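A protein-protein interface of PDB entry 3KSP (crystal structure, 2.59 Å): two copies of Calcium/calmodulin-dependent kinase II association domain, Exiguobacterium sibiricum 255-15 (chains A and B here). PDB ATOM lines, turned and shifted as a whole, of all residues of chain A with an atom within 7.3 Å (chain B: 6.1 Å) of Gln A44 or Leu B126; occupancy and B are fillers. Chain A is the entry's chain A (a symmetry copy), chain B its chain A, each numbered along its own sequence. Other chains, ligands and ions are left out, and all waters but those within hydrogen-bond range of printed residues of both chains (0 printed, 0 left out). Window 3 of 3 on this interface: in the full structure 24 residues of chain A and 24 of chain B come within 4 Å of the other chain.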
ATOM      1  N   ILE A  41     -15.394 -27.291 -12.699  1.00  0.00           N
ATOM      2  CA  ILE A  41     -16.686 -26.636 -12.892  1.00  0.00           C
ATOM      3  C   ILE A  41     -17.746 -27.234 -11.947  1.00  0.00           C
ATOM      4  O   ILE A  41     -18.019 -28.425 -12.004  1.00  0.00           O
ATOM      5  CB  ILE A  41     -17.130 -26.720 -14.353  1.00  0.00           C
ATOM      6  CG1 ILE A  41     -16.227 -25.830 -15.235  1.00  0.00           C
ATOM      7  CG2 ILE A  41     -18.585 -26.221 -14.517  1.00  0.00           C
ATOM      8  CD1 ILE A  41     -14.838 -26.305 -15.419  1.00  0.00           C
ATOM      9  N   ASP A  42     -18.312 -26.424 -11.054  1.00  0.00           N
ATOM     10  CA  ASP A  42     -19.333 -26.908 -10.136  1.00  0.00           C
ATOM     11  C   ASP A  42     -20.689 -26.963 -10.842  1.00  0.00           C
ATOM     12  O   ASP A  42     -20.811 -26.528 -11.967  1.00  0.00           O
ATOM     13  CB  ASP A  42     -19.365 -26.088  -8.816  1.00  0.00           C
ATOM     14  CG  ASP A  42     -20.096 -24.731  -8.936  1.00  0.00           C
ATOM     15  OD1 ASP A  42     -20.597 -24.358 -10.020  1.00  0.00           O
ATOM     16  OD2 ASP A  42     -20.159 -24.031  -7.899  1.00  0.00           O
ATOM     17  N   GLY A  43     -21.701 -27.491 -10.157  1.00  0.00           N
ATOM     18  CA  GLY A  43     -23.021 -27.686 -10.720  1.00  0.00           C
ATOM     19  C   GLY A  43     -23.809 -26.454 -11.075  1.00  0.00           C
ATOM     20  O   GLY A  43     -24.870 -26.609 -11.656  1.00  0.00           O
ATOM     21  N   GLN A  44     -23.339 -25.250 -10.709  1.00  0.00           N
ATOM     22  CA  GLN A  44     -23.895 -23.957 -11.202  1.00  0.00           C
ATOM     23  C   GLN A  44     -23.108 -23.436 -12.396  1.00  0.00           C
ATOM     24  O   GLN A  44     -23.437 -22.372 -12.934  1.00  0.00           O
ATOM     25  CB  GLN A  44     -23.794 -22.824 -10.161  1.00  0.00           C
ATOM     26  CG  GLN A  44     -24.428 -23.014  -8.798  1.00  0.00           C
ATOM     27  CD  GLN A  44     -25.862 -23.465  -8.895  1.00  0.00           C
ATOM     28  OE1 GLN A  44     -26.156 -24.685  -8.911  1.00  0.00           O
ATOM     29  NE2 GLN A  44     -26.780 -22.493  -8.935  1.00  0.00           N
ATOM     30  N   GLY A  45     -22.035 -24.136 -12.775  1.00  0.00           N
ATOM     31  CA  GLY A  45     -21.152 -23.682 -13.864  1.00  0.00           C
ATOM     32  C   GLY A  45     -20.052 -22.706 -13.486  1.00  0.00           C
ATOM     33  O   GLY A  45     -19.414 -22.130 -14.355  1.00  0.00           O
ATOM     34  N   ARG A  46     -19.828 -22.512 -12.195  1.00  0.00           N
ATOM     35  CA  ARG A  46     -18.718 -21.707 -11.730  1.00  0.00           C
ATOM     36  C   ARG A  46     -17.370 -22.465 -11.861  1.00  0.00           C
ATOM     37  O   ARG A  46     -17.240 -23.619 -11.450  1.00  0.00           O
ATOM     38  CB  ARG A  46     -18.956 -21.310 -10.281  1.00  0.00           C
ATOM     39  CG  ARG A  46     -17.937 -20.347  -9.710  1.00  0.00           C
ATOM     40  CD  ARG A  46     -18.295 -20.029  -8.267  1.00  0.00           C
ATOM     41  NE  ARG A  46     -17.198 -19.391  -7.541  1.00  0.00           N
ATOM     42  CZ  ARG A  46     -17.123 -19.308  -6.214  1.00  0.00           C
ATOM     43  NH1 ARG A  46     -18.074 -19.831  -5.437  1.00  0.00           N
ATOM     44  NH2 ARG A  46     -16.084 -18.706  -5.650  1.00  0.00           N
ATOM     45  N   GLN A  47     -16.382 -21.768 -12.415  1.00  0.00           N
ATOM     46  CA  GLN A  47     -15.053 -22.281 -12.682  1.00  0.00           C
ATOM     47  C   GLN A  47     -14.026 -21.938 -11.587  1.00  0.00           C
ATOM     48  O   GLN A  47     -13.813 -20.784 -11.246  1.00  0.00           O
ATOM     49  CB  GLN A  47     -14.573 -21.728 -14.033  1.00  0.00           C
ATOM     50  CG  GLN A  47     -13.093 -21.922 -14.313  1.00  0.00           C
ATOM     51  CD  GLN A  47     -12.834 -22.318 -15.730  1.00  0.00           C
ATOM     52  OE1 GLN A  47     -12.261 -23.385 -15.982  1.00  0.00           O
ATOM     53  NE2 GLN A  47     -13.274 -21.494 -16.675  1.00  0.00           N
ATOM     54  N   PHE A 103     -24.712 -35.557  -7.874  1.00  0.00           N
ATOM     55  CA  PHE A 103     -24.213 -35.023  -9.140  1.00  0.00           C
ATOM     56  C   PHE A 103     -23.831 -36.129 -10.086  1.00  0.00           C
ATOM     57  O   PHE A 103     -23.445 -37.226  -9.661  1.00  0.00           O
ATOM     58  CB  PHE A 103     -22.963 -34.137  -8.945  1.00  0.00           C
ATOM     59  CG  PHE A 103     -23.158 -32.990  -7.996  1.00  0.00           C
ATOM     60  CD1 PHE A 103     -23.716 -31.815  -8.422  1.00  0.00           C
ATOM     61  CD2 PHE A 103     -22.747 -33.085  -6.678  1.00  0.00           C
ATOM     62  CE1 PHE A 103     -23.884 -30.742  -7.534  1.00  0.00           C
ATOM     63  CE2 PHE A 103     -22.915 -32.024  -5.791  1.00  0.00           C
ATOM     64  CZ  PHE A 103     -23.470 -30.857  -6.228  1.00  0.00           C
ATOM     65  N   LEU A 123     -19.362 -30.834 -12.776  1.00  0.00           N
ATOM     66  CA  LEU A 123     -20.570 -31.337 -12.098  1.00  0.00           C
ATOM     67  C   LEU A 123     -21.872 -30.950 -12.836  1.00  0.00           C
ATOM     68  O   LEU A 123     -22.011 -29.809 -13.321  1.00  0.00           O
ATOM     69  CB  LEU A 123     -20.671 -30.753 -10.669  1.00  0.00           C
ATOM     70  CG  LEU A 123     -19.634 -31.171  -9.637  1.00  0.00           C
ATOM     71  CD1 LEU A 123     -20.137 -30.679  -8.232  1.00  0.00           C
ATOM     72  CD2 LEU A 123     -19.306 -32.714  -9.711  1.00  0.00           C
ATOM     73  N   THR A 124     -22.815 -31.890 -12.897  1.00  0.00           N
ATOM     74  CA  THR A 124     -24.171 -31.574 -13.324  1.00  0.00           C
ATOM     75  C   THR A 124     -25.159 -32.065 -12.265  1.00  0.00           C
ATOM     76  O   THR A 124     -25.217 -33.260 -11.999  1.00  0.00           O
ATOM     77  CB  THR A 124     -24.510 -32.215 -14.679  1.00  0.00           C
ATOM     78  OG1 THR A 124     -23.547 -31.792 -15.638  1.00  0.00           O
ATOM     79  CG2 THR A 124     -25.959 -31.812 -15.133  1.00  0.00           C
ATOM     80  N   PRO A 125     -25.908 -31.151 -11.641  1.00  0.00           N
ATOM     81  CA  PRO A 125     -26.762 -31.520 -10.489  1.00  0.00           C
ATOM     82  C   PRO A 125     -27.798 -32.572 -10.824  1.00  0.00           C
ATOM     83  O   PRO A 125     -28.325 -32.562 -11.926  1.00  0.00           O
ATOM     84  CB  PRO A 125     -27.459 -30.208 -10.127  1.00  0.00           C
ATOM     85  CG  PRO A 125     -26.602 -29.153 -10.680  1.00  0.00           C
ATOM     86  CD  PRO A 125     -25.946 -29.703 -11.907  1.00  0.00           C
ATOM     87  N   ILE B  87     -19.079 -22.487 -23.717  1.00  0.00           N
ATOM     88  CA  ILE B  87     -20.321 -21.915 -23.203  1.00  0.00           C
ATOM     89  C   ILE B  87     -21.211 -21.704 -24.432  1.00  0.00           C
ATOM     90  O   ILE B  87     -20.843 -20.945 -25.347  1.00  0.00           O
ATOM     91  CB  ILE B  87     -20.102 -20.586 -22.435  1.00  0.00           C
ATOM     92  CG1 ILE B  87     -19.360 -20.837 -21.099  1.00  0.00           C
ATOM     93  CG2 ILE B  87     -21.436 -19.881 -22.215  1.00  0.00           C
ATOM     94  CD1 ILE B  87     -19.124 -19.551 -20.230  1.00  0.00           C
ATOM     95  N   VAL B  88     -22.357 -22.394 -24.465  1.00  0.00           N
ATOM     96  CA  VAL B  88     -23.303 -22.309 -25.594  1.00  0.00           C
ATOM     97  C   VAL B  88     -24.630 -21.702 -25.160  1.00  0.00           C
ATOM     98  O   VAL B  88     -25.077 -21.895 -24.031  1.00  0.00           O
ATOM     99  CB  VAL B  88     -23.607 -23.694 -26.208  1.00  0.00           C
ATOM    100  CG1 VAL B  88     -22.454 -24.172 -27.063  1.00  0.00           C
ATOM    101  CG2 VAL B  88     -23.931 -24.691 -25.119  1.00  0.00           C
ATOM    102  N   GLY B 101     -31.761 -21.637 -23.716  1.00  0.00           N
ATOM    103  CA  GLY B 101     -31.048 -22.165 -22.559  1.00  0.00           C
ATOM    104  C   GLY B 101     -29.563 -22.051 -22.774  1.00  0.00           C
ATOM    105  O   GLY B 101     -29.071 -22.289 -23.881  1.00  0.00           O
ATOM    106  N   ARG B 102     -28.860 -21.639 -21.723  1.00  0.00           N
ATOM    107  CA  ARG B 102     -27.403 -21.539 -21.761  1.00  0.00           C
ATOM    108  C   ARG B 102     -26.739 -22.650 -20.951  1.00  0.00           C
ATOM    109  O   ARG B 102     -27.266 -23.102 -19.955  1.00  0.00           O
ATOM    110  CB  ARG B 102     -26.967 -20.179 -21.254  1.00  0.00           C
ATOM    111  CG  ARG B 102     -27.385 -19.095 -22.162  1.00  0.00           C
ATOM    112  CD  ARG B 102     -26.932 -17.718 -21.707  1.00  0.00           C
ATOM    113  NE  ARG B 102     -25.477 -17.567 -21.639  1.00  0.00           N
ATOM    114  CZ  ARG B 102     -24.768 -17.536 -20.510  1.00  0.00           C
ATOM    115  NH1 ARG B 102     -25.349 -17.662 -19.316  1.00  0.00           N
ATOM    116  NH2 ARG B 102     -23.455 -17.382 -20.564  1.00  0.00           N
ATOM    117  N   PHE B 103     -25.576 -23.099 -21.402  1.00  0.00           N
ATOM    118  CA  PHE B 103     -24.898 -24.218 -20.751  1.00  0.00           C
ATOM    119  C   PHE B 103     -23.403 -24.046 -20.784  1.00  0.00           C
ATOM    120  O   PHE B 103     -22.855 -23.412 -21.696  1.00  0.00           O
ATOM    121  CB  PHE B 103     -25.217 -25.567 -21.432  1.00  0.00           C
ATOM    122  CG  PHE B 103     -26.680 -25.889 -21.515  1.00  0.00           C
ATOM    123  CD1 PHE B 103     -27.333 -26.462 -20.457  1.00  0.00           C
ATOM    124  CD2 PHE B 103     -27.394 -25.644 -22.676  1.00  0.00           C
ATOM    125  CE1 PHE B 103     -28.698 -26.772 -20.545  1.00  0.00           C
ATOM    126  CE2 PHE B 103     -28.750 -25.946 -22.767  1.00  0.00           C
ATOM    127  CZ  PHE B 103     -29.390 -26.520 -21.708  1.00  0.00           C
ATOM    128  N   ARG B 104     -22.766 -24.594 -19.753  1.00  0.00           N
ATOM    129  CA  ARG B 104     -21.337 -24.835 -19.776  1.00  0.00           C
ATOM    130  C   ARG B 104     -21.216 -26.286 -20.191  1.00  0.00           C
ATOM    131  O   ARG B 104     -21.770 -27.168 -19.538  1.00  0.00           O
ATOM    132  CB  ARG B 104     -20.730 -24.589 -18.394  1.00  0.00           C
ATOM    133  CG  ARG B 104     -19.272 -24.947 -18.263  1.00  0.00           C
ATOM    134  CD  ARG B 104     -18.417 -24.372 -19.380  1.00  0.00           C
ATOM    135  NE  ARG B 104     -17.016 -24.714 -19.153  1.00  0.00           N
ATOM    136  CZ  ARG B 104     -16.095 -23.855 -18.729  1.00  0.00           C
ATOM    137  NH1 ARG B 104     -16.425 -22.587 -18.533  1.00  0.00           N
ATOM    138  NH2 ARG B 104     -14.850 -24.257 -18.518  1.00  0.00           N
ATOM    139  N   THR B 124     -23.926 -28.529 -18.229  1.00  0.00           N
ATOM    140  CA  THR B 124     -24.268 -28.001 -16.917  1.00  0.00           C
ATOM    141  C   THR B 124     -24.986 -26.661 -17.086  1.00  0.00           C
ATOM    142  O   THR B 124     -24.406 -25.726 -17.624  1.00  0.00           O
ATOM    143  CB  THR B 124     -23.025 -27.810 -16.033  1.00  0.00           C
ATOM    144  OG1 THR B 124     -22.339 -29.053 -15.934  1.00  0.00           O
ATOM    145  CG2 THR B 124     -23.435 -27.288 -14.610  1.00  0.00           C
ATOM    146  N   PRO B 125     -26.250 -26.575 -16.659  1.00  0.00           N
ATOM    147  CA  PRO B 125     -27.070 -25.372 -16.938  1.00  0.00           C
ATOM    148  C   PRO B 125     -26.478 -24.100 -16.372  1.00  0.00           C
ATOM    149  O   PRO B 125     -25.895 -24.138 -15.298  1.00  0.00           O
ATOM    150  CB  PRO B 125     -28.398 -25.678 -16.243  1.00  0.00           C
ATOM    151  CG  PRO B 125     -28.437 -27.139 -16.117  1.00  0.00           C
ATOM    152  CD  PRO B 125     -27.028 -27.617 -15.968  1.00  0.00           C
ATOM    153  N   LEU B 126     -26.577 -23.011 -17.115  1.00  0.00           N
ATOM    154  CA  LEU B 126     -26.195 -21.668 -16.644  1.00  0.00           C
ATOM    155  C   LEU B 126     -27.458 -20.787 -16.656  1.00  0.00           C
ATOM    156  O   LEU B 126     -28.427 -21.064 -17.407  1.00  0.00           O
ATOM    157  CB  LEU B 126     -25.139 -21.027 -17.571  1.00  0.00           C
ATOM    158  CG  LEU B 126     -23.723 -21.615 -17.642  1.00  0.00           C
ATOM    159  CD1 LEU B 126     -22.859 -20.874 -18.668  1.00  0.00           C
ATOM    160  CD2 LEU B 126     -23.105 -21.539 -16.283  1.00  0.00           C
ATOM    161  N   ASP B 127     -27.443 -19.722 -15.863  1.00  0.00           N
ATOM    162  CA  ASP B 127     -28.527 -18.729 -15.927  1.00  0.00           C
ATOM    163  C   ASP B 127     -28.650 -18.010 -17.302  1.00  0.00           C
ATOM    164  O   ASP B 127     -27.639 -17.799 -17.997  1.00  0.00           O
ATOM    165  CB  ASP B 127     -28.357 -17.677 -14.825  1.00  0.00           C
ATOM    166  CG  ASP B 127     -28.548 -18.249 -13.442  1.00  0.00           C
ATOM    167  OD1 ASP B 127     -29.154 -19.334 -13.318  1.00  0.00           O
ATOM    168  OD2 ASP B 127     -28.095 -17.599 -12.481  1.00  0.00           O
ATOM    169  N   PRO B 128     -29.896 -17.626 -17.691  1.00  0.00           N
ATOM    170  CA  PRO B 128     -30.125 -16.897 -18.960  1.00  0.00           C
ATOM    171  C   PRO B 128     -29.387 -15.539 -19.037  1.00  0.00           C
ATOM    172  O   PRO B 128     -29.088 -14.958 -17.995  1.00  0.00           O
ATOM    173  CB  PRO B 128     -31.653 -16.693 -18.972  1.00  0.00           C
ATOM    174  CG  PRO B 128     -32.107 -16.859 -17.535  1.00  0.00           C
ATOM    175  CD  PRO B 128     -31.167 -17.877 -16.968  1.00  0.00           C
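The side-chain hydroxyl (OG1) of Thr B124 is in hydrogen-bond range of the backbone carbonyl oxygen (O) of Leu A123 (2.7 Å).
The side-chain hydroxyl of Thr A124 is in hydrogen-bond range of the side-chain hydroxyl of Thr B124 (3.0 Å).
N of Leu B126 sits at hydrogen-bond distance from O of Arg B102, at 2.9 Å.
The backbone carbonyl oxygen (O) of Arg B104 sits at hydrogen-bond distance from the backbone NH (N) of Thr B124.
N of Leu A123 sits at hydrogen-bond distance from O of Ile A41, 2.9 Å away.
The side-chain carboxylate of Asp A42 sits at hydrogen-bond distance from the backbone NH of Gln A44 (3.0 Å).
N of Gly A45 sits at hydrogen-bond distance from OD1 of Asp A42 (3.1 Å).
The side-chain carboxylate of Asp A42 lies within hydrogen-bond range of the backbone NH of Arg A46 (3.0 Å).
Among the printed residues, merely in contact across the chains: Gly A43 with Thr B124 (3.4 Å), Gln A44 with Leu B126 (3.5 Å), Gln A47 with Arg B104 (3.7 Å), Ile A41 with Arg B104 (3.7 Å), Gly A45 with Leu B126 (3.8 Å), Asp A42 with Thr B124 (3.8 Å), Gln A44 with Pro B125 (3.8 Å) and Gly A45 with Thr B124 (3.9 Å).
Gln A44 touches two residues of chain B.
Of chain A, only Gln A44 and Gly A45 come within 4 Å of Leu B126.
Printed residues of chain B within 4 Å of Leu A123: Thr B124 (2.7 Å).
Printed residues of chain B within 4 Å of Asp A42: Thr B124.
Of the printed residues of chain A, Thr B124 touches Asp A42 (3.8 Å), Gly A43 (3.4 Å), Gly A45 (3.9 Å), Leu A123 (2.7 Å) and Thr A124 (3.0 Å).
Of the printed residues of chain B, Ile A41 touches Arg B104 (3.7 Å).
Pro B128 touches none of the printed residues of chain A.
The nearest residue of chain B that does not touch Gln A44 is Thr B124 (4.4 Å).
The nearest residue of chain A that does not touch Leu B126 is Arg A46 (5.3 Å).
The nearest printed residue of chain B that does not touch Gly A43 is Pro B125 (4.5 Å).
Of the 11 printed residues of chain A, 8 touch a printed residue of chain B.
Hydrophobic or aromatic side chains of chain A within 4 Å of the printed part of chain B: Ile A41.
Of the 11 printed residues of chain B, 4 touch a printed residue of chain A.
Printed residues of chain B that touch a printed residue of chain A: Arg B104, Thr B124, Pro B125 and Leu B126.
Among the printed residues, 10 pairs touch across the chains.
Among the printed residues, no Asp or Glu carboxylate lies within 4 Å of a Lys or Arg side-chain nitrogen of the other chain.
Thr A124 touches its own counterpart, Thr B124.
Positions printed for both chains: 103, 124 and 125.
Of the 10 pairs that touch across the chains among the printed residues, 1 has its exchanged pair printed and touching as well.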
